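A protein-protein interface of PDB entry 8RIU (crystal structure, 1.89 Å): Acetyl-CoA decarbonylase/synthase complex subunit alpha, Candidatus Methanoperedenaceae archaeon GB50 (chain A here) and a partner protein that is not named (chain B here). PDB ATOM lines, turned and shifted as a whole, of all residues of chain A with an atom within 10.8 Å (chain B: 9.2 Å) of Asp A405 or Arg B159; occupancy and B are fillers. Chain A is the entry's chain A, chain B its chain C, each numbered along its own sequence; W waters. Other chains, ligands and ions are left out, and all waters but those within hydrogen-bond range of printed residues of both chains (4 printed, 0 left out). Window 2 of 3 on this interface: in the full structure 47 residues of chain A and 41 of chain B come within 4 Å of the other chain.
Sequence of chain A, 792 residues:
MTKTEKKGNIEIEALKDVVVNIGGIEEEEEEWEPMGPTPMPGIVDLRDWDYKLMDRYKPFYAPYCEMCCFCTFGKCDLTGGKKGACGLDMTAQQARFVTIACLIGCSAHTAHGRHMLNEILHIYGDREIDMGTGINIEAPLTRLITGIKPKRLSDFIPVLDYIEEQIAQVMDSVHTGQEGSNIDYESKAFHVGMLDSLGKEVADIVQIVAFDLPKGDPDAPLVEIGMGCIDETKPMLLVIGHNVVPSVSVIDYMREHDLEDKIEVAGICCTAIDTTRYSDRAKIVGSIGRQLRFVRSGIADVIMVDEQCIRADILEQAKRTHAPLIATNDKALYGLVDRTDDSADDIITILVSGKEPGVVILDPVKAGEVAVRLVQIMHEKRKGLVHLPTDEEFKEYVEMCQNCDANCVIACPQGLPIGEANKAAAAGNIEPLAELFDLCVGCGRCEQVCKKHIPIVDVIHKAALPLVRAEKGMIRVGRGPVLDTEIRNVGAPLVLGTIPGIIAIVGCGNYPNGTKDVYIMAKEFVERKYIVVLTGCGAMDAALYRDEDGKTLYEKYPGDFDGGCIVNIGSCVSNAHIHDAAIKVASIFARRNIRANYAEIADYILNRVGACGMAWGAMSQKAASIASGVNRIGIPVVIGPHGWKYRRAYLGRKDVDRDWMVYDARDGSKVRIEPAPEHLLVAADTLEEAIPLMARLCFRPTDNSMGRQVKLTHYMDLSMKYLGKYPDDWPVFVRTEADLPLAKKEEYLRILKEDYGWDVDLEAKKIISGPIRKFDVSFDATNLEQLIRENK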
ATOM      1  N   CYS A 401      32.723  12.802   3.799  1.00  0.00           N
ATOM      2  CA  CYS A 401      31.893  11.819   3.114  1.00  0.00           C
ATOM      3  C   CYS A 401      30.534  11.723   3.796  1.00  0.00           C
ATOM      4  O   CYS A 401      30.440  11.715   5.025  1.00  0.00           O
ATOM      5  CB  CYS A 401      32.592  10.460   3.111  1.00  0.00           C
ATOM      6  SG  CYS A 401      31.544   9.062   2.647  1.00  0.00           S
ATOM      7  N   GLN A 402      29.474  11.677   2.991  1.00  0.00           N
ATOM      8  CA  GLN A 402      28.108  11.639   3.501  1.00  0.00           C
ATOM      9  C   GLN A 402      27.566  10.217   3.651  1.00  0.00           C
ATOM     10  O   GLN A 402      26.382  10.052   3.969  1.00  0.00           O
ATOM     11  CB  GLN A 402      27.179  12.454   2.589  1.00  0.00           C
ATOM     12  CG  GLN A 402      27.550  13.945   2.474  1.00  0.00           C
ATOM     13  CD  GLN A 402      26.495  14.781   1.757  1.00  0.00           C
ATOM     14  OE1 GLN A 402      25.637  14.249   1.044  1.00  0.00           O
ATOM     15  NE2 GLN A 402      26.542  16.103   1.961  1.00  0.00           N
ATOM     16  N   ASN A 403      28.399   9.196   3.453  1.00  0.00           N
ATOM     17  CA  ASN A 403      27.975   7.797   3.584  1.00  0.00           C
ATOM     18  C   ASN A 403      26.714   7.551   2.769  1.00  0.00           C
ATOM     19  O   ASN A 403      25.736   6.977   3.246  1.00  0.00           O
ATOM     20  CB  ASN A 403      27.759   7.400   5.052  1.00  0.00           C
ATOM     21  CG  ASN A 403      27.920   5.896   5.284  1.00  0.00           C
ATOM     22  OD1 ASN A 403      28.298   5.150   4.371  1.00  0.00           O
ATOM     23  ND2 ASN A 403      27.614   5.441   6.499  1.00  0.00           N
ATOM     24  N   CYS A 404      26.732   8.080   1.553  1.00  0.00           N
ATOM     25  CA  CYS A 404      25.567   7.979   0.643  1.00  0.00           C
ATOM     26  C   CYS A 404      25.097   6.530   0.524  1.00  0.00           C
ATOM     27  O   CYS A 404      25.934   5.641   0.383  1.00  0.00           O
ATOM     28  CB  CYS A 404      25.945   8.547  -0.721  1.00  0.00           C
ATOM     29  SG  CYS A 404      26.698  10.189  -0.682  1.00  0.00           S
ATOM     30  N   ASP A 405      23.786   6.333   0.555  1.00  0.00           N
ATOM     31  CA  ASP A 405      23.205   4.975   0.447  1.00  0.00           C
ATOM     32  C   ASP A 405      23.550   4.322  -0.888  1.00  0.00           C
ATOM     33  O   ASP A 405      23.856   3.138  -0.870  1.00  0.00           O
ATOM     34  CB  ASP A 405      21.683   5.050   0.528  1.00  0.00           C
ATOM     35  CG  ASP A 405      21.041   4.259   1.649  1.00  0.00           C
ATOM     36  OD1 ASP A 405      21.767   3.812   2.544  1.00  0.00           O
ATOM     37  OD2 ASP A 405      19.810   4.114   1.614  1.00  0.00           O
ATOM     38  N   ALA A 406      23.520   5.078  -1.988  1.00  0.00           N
ATOM     39  CA  ALA A 406      23.657   4.453  -3.324  1.00  0.00           C
ATOM     40  C   ALA A 406      24.253   5.385  -4.386  1.00  0.00           C
ATOM     41  O   ALA A 406      23.617   5.576  -5.424  1.00  0.00           O
ATOM     42  CB  ALA A 406      22.311   3.942  -3.747  1.00  0.00           C
ATOM     43  N   ASN A 407      25.448   5.899  -4.146  1.00  0.00           N
ATOM     44  CA  ASN A 407      26.138   6.691  -5.156  1.00  0.00           C
ATOM     45  C   ASN A 407      27.403   5.923  -5.553  1.00  0.00           C
ATOM     46  O   ASN A 407      27.335   5.062  -6.432  1.00  0.00           O
ATOM     47  CB  ASN A 407      26.414   8.110  -4.647  1.00  0.00           C
ATOM     48  CG  ASN A 407      25.178   8.994  -4.701  1.00  0.00           C
ATOM     49  OD1 ASN A 407      24.367   8.886  -5.623  1.00  0.00           O
ATOM     50  ND2 ASN A 407      25.032   9.881  -3.719  1.00  0.00           N
ATOM     51  N   CYS A 408      28.539   6.202  -4.920  1.00  0.00           N
ATOM     52  CA  CYS A 408      29.832   5.573  -5.318  1.00  0.00           C
ATOM     53  C   CYS A 408      29.715   4.042  -5.393  1.00  0.00           C
ATOM     54  O   CYS A 408      30.206   3.473  -6.366  1.00  0.00           O
ATOM     55  CB  CYS A 408      30.954   6.006  -4.375  1.00  0.00           C
ATOM     56  SG  CYS A 408      30.653   5.666  -2.626  1.00  0.00           S
ATOM     57  N   VAL A 409      29.053   3.417  -4.427  1.00  0.00           N
ATOM     58  CA  VAL A 409      28.950   1.930  -4.397  1.00  0.00           C
ATOM     59  C   VAL A 409      28.236   1.451  -5.666  1.00  0.00           C
ATOM     60  O   VAL A 409      28.611   0.414  -6.193  1.00  0.00           O
ATOM     61  CB  VAL A 409      28.245   1.439  -3.119  1.00  0.00           C
ATOM     62  CG1 VAL A 409      26.863   2.048  -2.957  1.00  0.00           C
ATOM     63  CG2 VAL A 409      28.187  -0.078  -3.046  1.00  0.00           C
ATOM     64  N   ILE A 410      27.262   2.224  -6.135  1.00  0.00           N
ATOM     65  CA  ILE A 410      26.476   1.824  -7.335  1.00  0.00           C
ATOM     66  C   ILE A 410      27.338   2.017  -8.590  1.00  0.00           C
ATOM     67  O   ILE A 410      27.198   1.222  -9.508  1.00  0.00           O
ATOM     68  CB  ILE A 410      25.158   2.622  -7.412  1.00  0.00           C
ATOM     69  CG1 ILE A 410      24.324   2.450  -6.142  1.00  0.00           C
ATOM     70  CG2 ILE A 410      24.366   2.249  -8.654  1.00  0.00           C
ATOM     71  CD1 ILE A 410      24.090   1.015  -5.756  1.00  0.00           C
ATOM     72  N   ALA A 411      28.192   3.040  -8.609  1.00  0.00           N
ATOM     73  CA  ALA A 411      29.026   3.236  -9.787  1.00  0.00           C
ATOM     74  C   ALA A 411      30.214   2.287  -9.823  1.00  0.00           C
ATOM     75  O   ALA A 411      30.849   2.157 -10.873  1.00  0.00           O
ATOM     76  CB  ALA A 411      29.528   4.679  -9.848  1.00  0.00           C
ATOM     77  N   CYS A 412      30.529   1.637  -8.712  1.00  0.00           N
ATOM     78  CA  CYS A 412      31.704   0.783  -8.639  1.00  0.00           C
ATOM     79  C   CYS A 412      31.398  -0.586  -9.236  1.00  0.00           C
ATOM     80  O   CYS A 412      30.417  -1.218  -8.840  1.00  0.00           O
ATOM     81  CB  CYS A 412      32.158   0.621  -7.190  1.00  0.00           C
ATOM     82  SG  CYS A 412      33.497  -0.610  -6.946  1.00  0.00           S
ATOM     83  N   GLY A 415      31.009  -2.991  -6.449  1.00  0.00           N
ATOM     84  CA  GLY A 415      30.126  -2.646  -5.343  1.00  0.00           C
ATOM     85  C   GLY A 415      30.828  -2.513  -4.008  1.00  0.00           C
ATOM     86  O   GLY A 415      30.297  -2.957  -2.984  1.00  0.00           O
ATOM     87  N   LEU A 416      32.001  -1.894  -3.991  1.00  0.00           N
ATOM     88  CA  LEU A 416      32.781  -1.820  -2.763  1.00  0.00           C
ATOM     89  C   LEU A 416      32.153  -0.852  -1.761  1.00  0.00           C
ATOM     90  O   LEU A 416      31.596   0.183  -2.151  1.00  0.00           O
ATOM     91  CB  LEU A 416      34.209  -1.393  -3.083  1.00  0.00           C
ATOM     92  CG  LEU A 416      35.005  -2.386  -3.937  1.00  0.00           C
ATOM     93  CD1 LEU A 416      36.454  -2.023  -3.922  1.00  0.00           C
ATOM     94  CD2 LEU A 416      34.834  -3.830  -3.476  1.00  0.00           C
ATOM     95  N   PRO A 417      32.228  -1.159  -0.441  1.00  0.00           N
ATOM     96  CA  PRO A 417      31.633  -0.316   0.612  1.00  0.00           C
ATOM     97  C   PRO A 417      32.470   0.924   0.948  1.00  0.00           C
ATOM     98  O   PRO A 417      32.950   1.010   2.051  1.00  0.00           O
ATOM     99  CB  PRO A 417      31.590  -1.277   1.804  1.00  0.00           C
ATOM    100  CG  PRO A 417      32.805  -2.131   1.635  1.00  0.00           C
ATOM    101  CD  PRO A 417      32.861  -2.357   0.144  1.00  0.00           C
ATOM    102  N   ILE A 418      32.597   1.850   0.001  1.00  0.00           N
ATOM    103  CA  ILE A 418      33.462   3.047   0.188  1.00  0.00           C
ATOM    104  C   ILE A 418      32.935   3.934   1.317  1.00  0.00           C
ATOM    105  O   ILE A 418      33.736   4.347   2.152  1.00  0.00           O
ATOM    106  CB  ILE A 418      33.577   3.818  -1.145  1.00  0.00           C
ATOM    107  CG1 ILE A 418      34.266   2.980  -2.223  1.00  0.00           C
ATOM    108  CG2 ILE A 418      34.260   5.160  -0.944  1.00  0.00           C
ATOM    109  CD1 ILE A 418      33.631   3.091  -3.586  1.00  0.00           C
ATOM    110  N   GLY A 419      31.640   4.221   1.313  1.00  0.00           N
ATOM    111  CA  GLY A 419      31.079   5.143   2.311  1.00  0.00           C
ATOM    112  C   GLY A 419      31.282   4.614   3.708  1.00  0.00           C
ATOM    113  O   GLY A 419      31.777   5.350   4.561  1.00  0.00           O
ATOM    114  N   GLU A 420      30.921   3.354   3.896  1.00  0.00           N
ATOM    115  CA  GLU A 420      31.059   2.751   5.241  1.00  0.00           C
ATOM    116  C   GLU A 420      32.545   2.696   5.607  1.00  0.00           C
ATOM    117  O   GLU A 420      32.864   2.909   6.776  1.00  0.00           O
ATOM    118  CB  GLU A 420      30.404   1.375   5.267  1.00  0.00           C
ATOM    119  CG  GLU A 420      28.974   1.372   4.776  1.00  0.00           C
ATOM    120  CD  GLU A 420      28.539   0.021   4.241  1.00  0.00           C
ATOM    121  OE1 GLU A 420      28.084  -0.814   5.042  1.00  0.00           O
ATOM    122  OE2 GLU A 420      28.674  -0.194   3.029  1.00  0.00           O
ATOM    123  N   LYS A 423      33.583   6.250   6.761  1.00  0.00           N
ATOM    124  CA  LYS A 423      33.093   6.626   8.110  1.00  0.00           C
ATOM    125  C   LYS A 423      33.909   5.869   9.164  1.00  0.00           C
ATOM    126  O   LYS A 423      34.244   6.471  10.180  1.00  0.00           O
ATOM    127  CB  LYS A 423      31.585   6.384   8.198  1.00  0.00           C
ATOM    128  CG  LYS A 423      30.728   7.250   7.282  1.00  0.00           C
ATOM    129  CD  LYS A 423      31.429   8.481   6.755  1.00  0.00           C
ATOM    130  CE  LYS A 423      31.270   9.689   7.653  1.00  0.00           C
ATOM    131  NZ  LYS A 423      31.963  10.880   7.110  1.00  0.00           N
ATOM    132  N   VAL A 449      30.691  10.156  -9.470  1.00  0.00           N
ATOM    133  CA  VAL A 449      29.351  10.336  -8.924  1.00  0.00           C
ATOM    134  C   VAL A 449      29.372  10.915  -7.512  1.00  0.00           C
ATOM    135  O   VAL A 449      28.308  11.046  -6.883  1.00  0.00           O
ATOM    136  CB  VAL A 449      28.574   9.004  -8.942  1.00  0.00           C
ATOM    137  CG1 VAL A 449      28.396   8.503 -10.380  1.00  0.00           C
ATOM    138  CG2 VAL A 449      29.289   7.961  -8.098  1.00  0.00           C
ATOM    139  N   ILE B   3      17.037   2.074  -8.280  1.00  0.00           N
ATOM    140  CA  ILE B   3      18.496   2.148  -8.559  1.00  0.00           C
ATOM    141  C   ILE B   3      19.070   0.746  -8.756  1.00  0.00           C
ATOM    142  O   ILE B   3      19.195   0.014  -7.776  1.00  0.00           O
ATOM    143  CB  ILE B   3      19.217   2.902  -7.429  1.00  0.00           C
ATOM    144  CG1 ILE B   3      18.598   4.279  -7.174  1.00  0.00           C
ATOM    145  CG2 ILE B   3      20.707   2.997  -7.712  1.00  0.00           C
ATOM    146  CD1 ILE B   3      19.008   4.893  -5.861  1.00  0.00           C
ATOM    147  N   PHE B   5      21.940  -1.959  -8.956  1.00  0.00           N
ATOM    148  CA  PHE B   5      23.208  -1.933  -8.176  1.00  0.00           C
ATOM    149  C   PHE B   5      24.358  -1.448  -9.057  1.00  0.00           C
ATOM    150  O   PHE B   5      25.278  -0.833  -8.526  1.00  0.00           O
ATOM    151  CB  PHE B   5      23.485  -3.280  -7.514  1.00  0.00           C
ATOM    152  CG  PHE B   5      24.477  -3.188  -6.386  1.00  0.00           C
ATOM    153  CD1 PHE B   5      24.169  -2.487  -5.235  1.00  0.00           C
ATOM    154  CD2 PHE B   5      25.727  -3.774  -6.490  1.00  0.00           C
ATOM    155  CE1 PHE B   5      25.083  -2.388  -4.201  1.00  0.00           C
ATOM    156  CE2 PHE B   5      26.637  -3.679  -5.453  1.00  0.00           C
ATOM    157  CZ  PHE B   5      26.314  -2.985  -4.312  1.00  0.00           C
ATOM    158  N   ASP B  45      25.361 -12.434   6.968  1.00  0.00           N
ATOM    159  CA  ASP B  45      24.195 -11.821   7.673  1.00  0.00           C
ATOM    160  C   ASP B  45      23.069 -12.821   7.960  1.00  0.00           C
ATOM    161  O   ASP B  45      21.903 -12.427   7.806  1.00  0.00           O
ATOM    162  CB  ASP B  45      23.629 -10.636   6.882  1.00  0.00           C
ATOM    163  CG  ASP B  45      24.669  -9.665   6.352  1.00  0.00           C
ATOM    164  OD1 ASP B  45      25.526  -9.236   7.143  1.00  0.00           O
ATOM    165  OD2 ASP B  45      24.612  -9.353   5.147  1.00  0.00           O
ATOM    166  N   ARG B 142      18.499  -8.032  -1.847  1.00  0.00           N
ATOM    167  CA  ARG B 142      18.592  -6.619  -1.395  1.00  0.00           C
ATOM    168  C   ARG B 142      18.798  -5.675  -2.580  1.00  0.00           C
ATOM    169  O   ARG B 142      18.926  -4.463  -2.337  1.00  0.00           O
ATOM    170  CB  ARG B 142      19.774  -6.474  -0.435  1.00  0.00           C
ATOM    171  CG  ARG B 142      21.006  -7.260  -0.865  1.00  0.00           C
ATOM    172  CD  ARG B 142      22.303  -6.644  -0.377  1.00  0.00           C
ATOM    173  NE  ARG B 142      22.395  -6.631   1.076  1.00  0.00           N
ATOM    174  CZ  ARG B 142      22.830  -7.644   1.815  1.00  0.00           C
ATOM    175  NH1 ARG B 142      23.311  -8.730   1.235  1.00  0.00           N
ATOM    176  NH2 ARG B 142      22.788  -7.566   3.134  1.00  0.00           N
ATOM    177  N   ASN B 154      16.485  -1.202  -4.191  1.00  0.00           N
ATOM    178  CA  ASN B 154      17.834  -1.360  -3.599  1.00  0.00           C
ATOM    179  C   ASN B 154      17.770  -1.107  -2.093  1.00  0.00           C
ATOM    180  O   ASN B 154      17.193  -0.087  -1.693  1.00  0.00           O
ATOM    181  CB  ASN B 154      18.868  -0.425  -4.228  1.00  0.00           C
ATOM    182  CG  ASN B 154      20.267  -0.668  -3.705  1.00  0.00           C
ATOM    183  OD1 ASN B 154      20.875  -1.691  -4.002  1.00  0.00           O
ATOM    184  ND2 ASN B 154      20.780   0.265  -2.922  1.00  0.00           N
ATOM    185  N   ILE B 155      18.329  -2.017  -1.301  1.00  0.00           N
ATOM    186  CA  ILE B 155      18.418  -1.794   0.168  1.00  0.00           C
ATOM    187  C   ILE B 155      19.906  -1.828   0.528  1.00  0.00           C
ATOM    188  O   ILE B 155      20.495  -2.899   0.446  1.00  0.00           O
ATOM    189  CB  ILE B 155      17.586  -2.815   0.971  1.00  0.00           C
ATOM    190  CG1 ILE B 155      16.123  -2.846   0.524  1.00  0.00           C
ATOM    191  CG2 ILE B 155      17.715  -2.555   2.462  1.00  0.00           C
ATOM    192  CD1 ILE B 155      15.340  -3.994   1.106  1.00  0.00           C
ATOM    193  N   SER B 156      20.466  -0.677   0.875  1.00  0.00           N
ATOM    194  CA  SER B 156      21.904  -0.565   1.206  1.00  0.00           C
ATOM    195  C   SER B 156      22.326  -1.582   2.267  1.00  0.00           C
ATOM    196  O   SER B 156      21.504  -1.946   3.114  1.00  0.00           O
ATOM    197  CB  SER B 156      22.234   0.818   1.694  1.00  0.00           C
ATOM    198  OG  SER B 156      21.801   1.009   3.025  1.00  0.00           O
ATOM    199  N   ARG B 157      23.593  -1.980   2.219  1.00  0.00           N
ATOM    200  CA  ARG B 157      24.105  -2.928   3.199  1.00  0.00           C
ATOM    201  C   ARG B 157      24.033  -2.397   4.620  1.00  0.00           C
ATOM    202  O   ARG B 157      23.870  -3.179   5.564  1.00  0.00           O
ATOM    203  CB  ARG B 157      25.541  -3.315   2.854  1.00  0.00           C
ATOM    204  CG  ARG B 157      25.598  -4.403   1.823  1.00  0.00           C
ATOM    205  CD  ARG B 157      26.938  -5.070   1.756  1.00  0.00           C
ATOM    206  NE  ARG B 157      26.893  -6.148   0.777  1.00  0.00           N
ATOM    207  CZ  ARG B 157      26.613  -7.411   1.065  1.00  0.00           C
ATOM    208  NH1 ARG B 157      26.367  -7.800   2.307  1.00  0.00           N
ATOM    209  NH2 ARG B 157      26.578  -8.306   0.081  1.00  0.00           N
ATOM    210  N   LYS B 158      24.158  -1.084   4.800  1.00  0.00           N
ATOM    211  CA  LYS B 158      24.027  -0.543   6.145  1.00  0.00           C
ATOM    212  C   LYS B 158      22.579  -0.540   6.621  1.00  0.00           C
ATOM    213  O   LYS B 158      22.333  -0.295   7.807  1.00  0.00           O
ATOM    214  CB  LYS B 158      24.627   0.864   6.214  1.00  0.00           C
ATOM    215  CG  LYS B 158      24.113   1.848   5.181  1.00  0.00           C
ATOM    216  CD  LYS B 158      24.969   3.105   5.181  1.00  0.00           C
ATOM    217  CE  LYS B 158      24.492   4.129   4.163  1.00  0.00           C
ATOM    218  NZ  LYS B 158      23.219   4.800   4.549  1.00  0.00           N
ATOM    219  N   ARG B 159      21.624  -0.837   5.741  1.00  0.00           N
ATOM    220  CA  ARG B 159      20.227  -1.017   6.117  1.00  0.00           C
ATOM    221  C   ARG B 159      19.802  -2.479   5.984  1.00  0.00           C
ATOM    222  O   ARG B 159      18.648  -2.777   5.671  1.00  0.00           O
ATOM    223  CB  ARG B 159      19.343  -0.100   5.274  1.00  0.00           C
ATOM    224  CG  ARG B 159      19.698   1.386   5.433  1.00  0.00           C
ATOM    225  CD  ARG B 159      19.056   2.284   4.370  1.00  0.00           C
ATOM    226  NE  ARG B 159      17.610   2.371   4.535  1.00  0.00           N
ATOM    227  CZ  ARG B 159      16.824   3.235   3.904  1.00  0.00           C
ATOM    228  NH1 ARG B 159      17.315   4.133   3.065  1.00  0.00           N
ATOM    229  NH2 ARG B 159      15.514   3.202   4.130  1.00  0.00           N
ATOM    230  N   THR B 160      20.734  -3.406   6.230  1.00  0.00           N
ATOM    231  CA  THR B 160      20.437  -4.828   6.062  1.00  0.00           C
ATOM    232  C   THR B 160      19.332  -5.289   7.004  1.00  0.00           C
ATOM    233  O   THR B 160      18.568  -6.202   6.661  1.00  0.00           O
ATOM    234  CB  THR B 160      21.707  -5.656   6.282  1.00  0.00           C
ATOM    235  OG1 THR B 160      22.616  -5.431   5.195  1.00  0.00           O
ATOM    236  CG2 THR B 160      21.393  -7.156   6.374  1.00  0.00           C
ATOM    237  N   ASP B 161      19.239  -4.699   8.197  1.00  0.00           N
ATOM    238  CA  ASP B 161      18.143  -5.039   9.098  1.00  0.00           C
ATOM    239  C   ASP B 161      16.796  -4.839   8.414  1.00  0.00           C
ATOM    240  O   ASP B 161      15.880  -5.650   8.579  1.00  0.00           O
ATOM    241  CB  ASP B 161      18.239  -4.201  10.376  1.00  0.00           C
ATOM    242  CG  ASP B 161      18.079  -2.710  10.118  1.00  0.00           C
ATOM    243  OD1 ASP B 161      18.186  -2.285   8.949  1.00  0.00           O
ATOM    244  OD2 ASP B 161      17.848  -1.959  11.087  1.00  0.00           O
ATOM    245  N   GLU B 162      16.678  -3.792   7.602  1.00  0.00           N
ATOM    246  CA  GLU B 162      15.424  -3.534   6.850  1.00  0.00           C
ATOM    247  C   GLU B 162      15.200  -4.645   5.819  1.00  0.00           C
ATOM    248  O   GLU B 162      14.064  -5.108   5.691  1.00  0.00           O
ATOM    249  CB  GLU B 162      15.464  -2.157   6.189  1.00  0.00           C
ATOM    250  CG  GLU B 162      15.447  -0.997   7.162  1.00  0.00           C
ATOM    251  CD  GLU B 162      15.686   0.347   6.497  1.00  0.00           C
ATOM    252  OE1 GLU B 162      14.996   0.645   5.510  1.00  0.00           O
ATOM    253  OE2 GLU B 162      16.568   1.079   6.959  1.00  0.00           O
ATOM    254  N   PHE B 163      16.257  -5.053   5.120  1.00  0.00           N
ATOM    255  CA  PHE B 163      16.145  -6.134   4.110  1.00  0.00           C
ATOM    256  C   PHE B 163      15.643  -7.412   4.786  1.00  0.00           C
ATOM    257  O   PHE B 163      14.792  -8.089   4.225  1.00  0.00           O
ATOM    258  CB  PHE B 163      17.493  -6.343   3.421  1.00  0.00           C
ATOM    259  CG  PHE B 163      17.606  -7.576   2.565  1.00  0.00           C
ATOM    260  CD1 PHE B 163      16.597  -7.923   1.684  1.00  0.00           C
ATOM    261  CD2 PHE B 163      18.729  -8.379   2.630  1.00  0.00           C
ATOM    262  CE1 PHE B 163      16.703  -9.059   0.901  1.00  0.00           C
ATOM    263  CE2 PHE B 163      18.838  -9.510   1.839  1.00  0.00           C
ATOM    264  CZ  PHE B 163      17.824  -9.849   0.977  1.00  0.00           C
ATOM    265  N   LYS B 164      16.161  -7.699   5.977  1.00  0.00           N
ATOM    266  CA  LYS B 164      15.790  -8.949   6.685  1.00  0.00           C
ATOM    267  C   LYS B 164      14.322  -8.898   7.123  1.00  0.00           C
ATOM    268  O   LYS B 164      13.679  -9.938   7.082  1.00  0.00           O
ATOM    269  CB  LYS B 164      16.743  -9.178   7.860  1.00  0.00           C
ATOM    270  CG  LYS B 164      18.160  -9.565   7.469  1.00  0.00           C
ATOM    271  CD  LYS B 164      18.885 -10.312   8.557  1.00  0.00           C
ATOM    272  CE  LYS B 164      20.267  -9.759   8.818  1.00  0.00           C
ATOM    273  NZ  LYS B 164      21.003 -10.575   9.809  1.00  0.00           N
ATOM    274  N   GLU B 165      13.817  -7.717   7.485  1.00  0.00           N
ATOM    275  CA  GLU B 165      12.375  -7.636   7.835  1.00  0.00           C
ATOM    276  C   GLU B 165      11.554  -7.962   6.590  1.00  0.00           C
ATOM    277  O   GLU B 165      10.589  -8.721   6.704  1.00  0.00           O
ATOM    278  CB  GLU B 165      12.021  -6.243   8.355  1.00  0.00           C
ATOM    279  CG  GLU B 165      12.854  -5.801   9.540  1.00  0.00           C
ATOM    280  CD  GLU B 165      12.769  -4.317   9.860  1.00  0.00           C
ATOM    281  OE1 GLU B 165      12.208  -3.568   9.041  1.00  0.00           O
ATOM    282  OE2 GLU B 165      13.263  -3.916  10.929  1.00  0.00           O
ATOM    283  N   MET B 166      11.960  -7.421   5.448  1.00  0.00           N
ATOM    284  CA  MET B 166      11.201  -7.648   4.196  1.00  0.00           C
ATOM    285  C   MET B 166      11.306  -9.116   3.770  1.00  0.00           C
ATOM    286  O   MET B 166      10.281  -9.692   3.398  1.00  0.00           O
ATOM    287  CB  MET B 166      11.719  -6.720   3.103  1.00  0.00           C
ATOM    288  CG  MET B 166      11.249  -5.298   3.301  1.00  0.00           C
ATOM    289  SD  MET B 166      12.256  -4.123   2.391  1.00  0.00           S
ATOM    290  CE  MET B 166      11.750  -4.501   0.716  1.00  0.00           C
HETATM  291  O   HOH W   1      19.019   1.745   0.740  1.00  0.00           O
HETATM  292  O   HOH W   2      25.795   0.245   2.870  1.00  0.00           O
HETATM  293  O   HOH W   3      23.416   0.550  -1.745  1.00  0.00           O
HETATM  294  O   HOH W   4      27.016  -2.936   6.597  1.00  0.00           O
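The side-chain carboxylate (OD1) of Asp A405 is in hydrogen-bond range of the side-chain hydroxyl (OG) of Ser B156 (2.8 Å). NZ of Lys B158 lies within salt-bridge range of OD1 of Asp A405, 2.7 Å away. OD2 of Asp A405 lies within salt-bridge range of NH1 of Arg B159 (2.9 Å). The backbone carbonyl oxygen of Phe B5 sits close to the backbone carbonyl oxygen of Ile A410, 3.0 Å away.
Of the 20 printed residues of chain A, 6 touch a printed residue of chain B. Hydrophobic or aromatic side chains of chain A that line the printed part of chain B: Val A409 and Ile A410. Among the printed residues, 9 pairs touch across the chains. Among the printed residues, Asp or Glu carboxylates within 4 Å of a Lys or Arg side-chain nitrogen of the other chain: Asp A405 with Lys B158 and Asp A405 with Arg B159.
The backbone NH (N) of Asn A403 lies close to the side-chain sulfur (SG) of Cys A401, 3.2 Å away. OD1 of Asn A403 lies close to O of Gly A419 (3.5 Å). N of Glu A420 is in hydrogen-bond range of OD1 of Asn A403 (3.2 Å). The side-chain sulfur (SG) of Cys A412 lies close to the backbone NH (N) of Gly A415, at 3.5 Å. The backbone NH (N) of Arg B159 lies close to the side-chain hydroxyl (OG) of Ser B156 (3.3 Å).
Water W1 lies within hydrogen-bond range of OD2 of Asp A405 (2.6 Å) and N of Ser B156 (2.8 Å). Water W3 lies within hydrogen-bond range of the backbone carbonyl oxygen (O) of Asp A405 and the side-chain amide nitrogen (ND2) of Asn B154. Water W2 lies within hydrogen-bond range of the backbone NH of Lys B158, the side-chain carboxylate of Glu A420 and the backbone NH of Arg B157.
Lys B158 touches Asn A403. Phe B5 touches Val A409. CG2 of Ile B3 touches CG2 of Ile A410, at 3.9 Å. Gly A415 touches Phe B5 (CA to CE2, 3.6 Å). Glu A420 touches Lys B158.
Of chain B, only Ser B156, Lys B158 and Arg B159 come within 4 Å of Asp A405. No residue of chain B comes within 4 Å of Cys A404. Ser B156 touches one residue of chain A. Lys B158 touches just these residues of chain A: Asn A403 (3.2 Å), Asp A405 (2.7 Å) and Glu A420 (3.9 Å). No residue of chain A comes within 4 Å of Thr B160. No residue of chain A comes within 4 Å of Glu B162. Of the printed residues of chain A, Ile B3 touches Ile A410. Printed residues of chain B within 4 Å of Asn A403: Lys B158 (3.2 Å). Printed residues of chain A within 4 Å of Phe B5: Val A409 (3.7 Å), Ile A410 (3.0 Å) and Gly A415 (3.6 Å). Asn A407 touches none of the printed residues of chain B. Ala A411 touches none of the printed residues of chain B. The nearest printed residue of chain B that does not touch Ile A410 is Asn B154 (4.4 Å).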
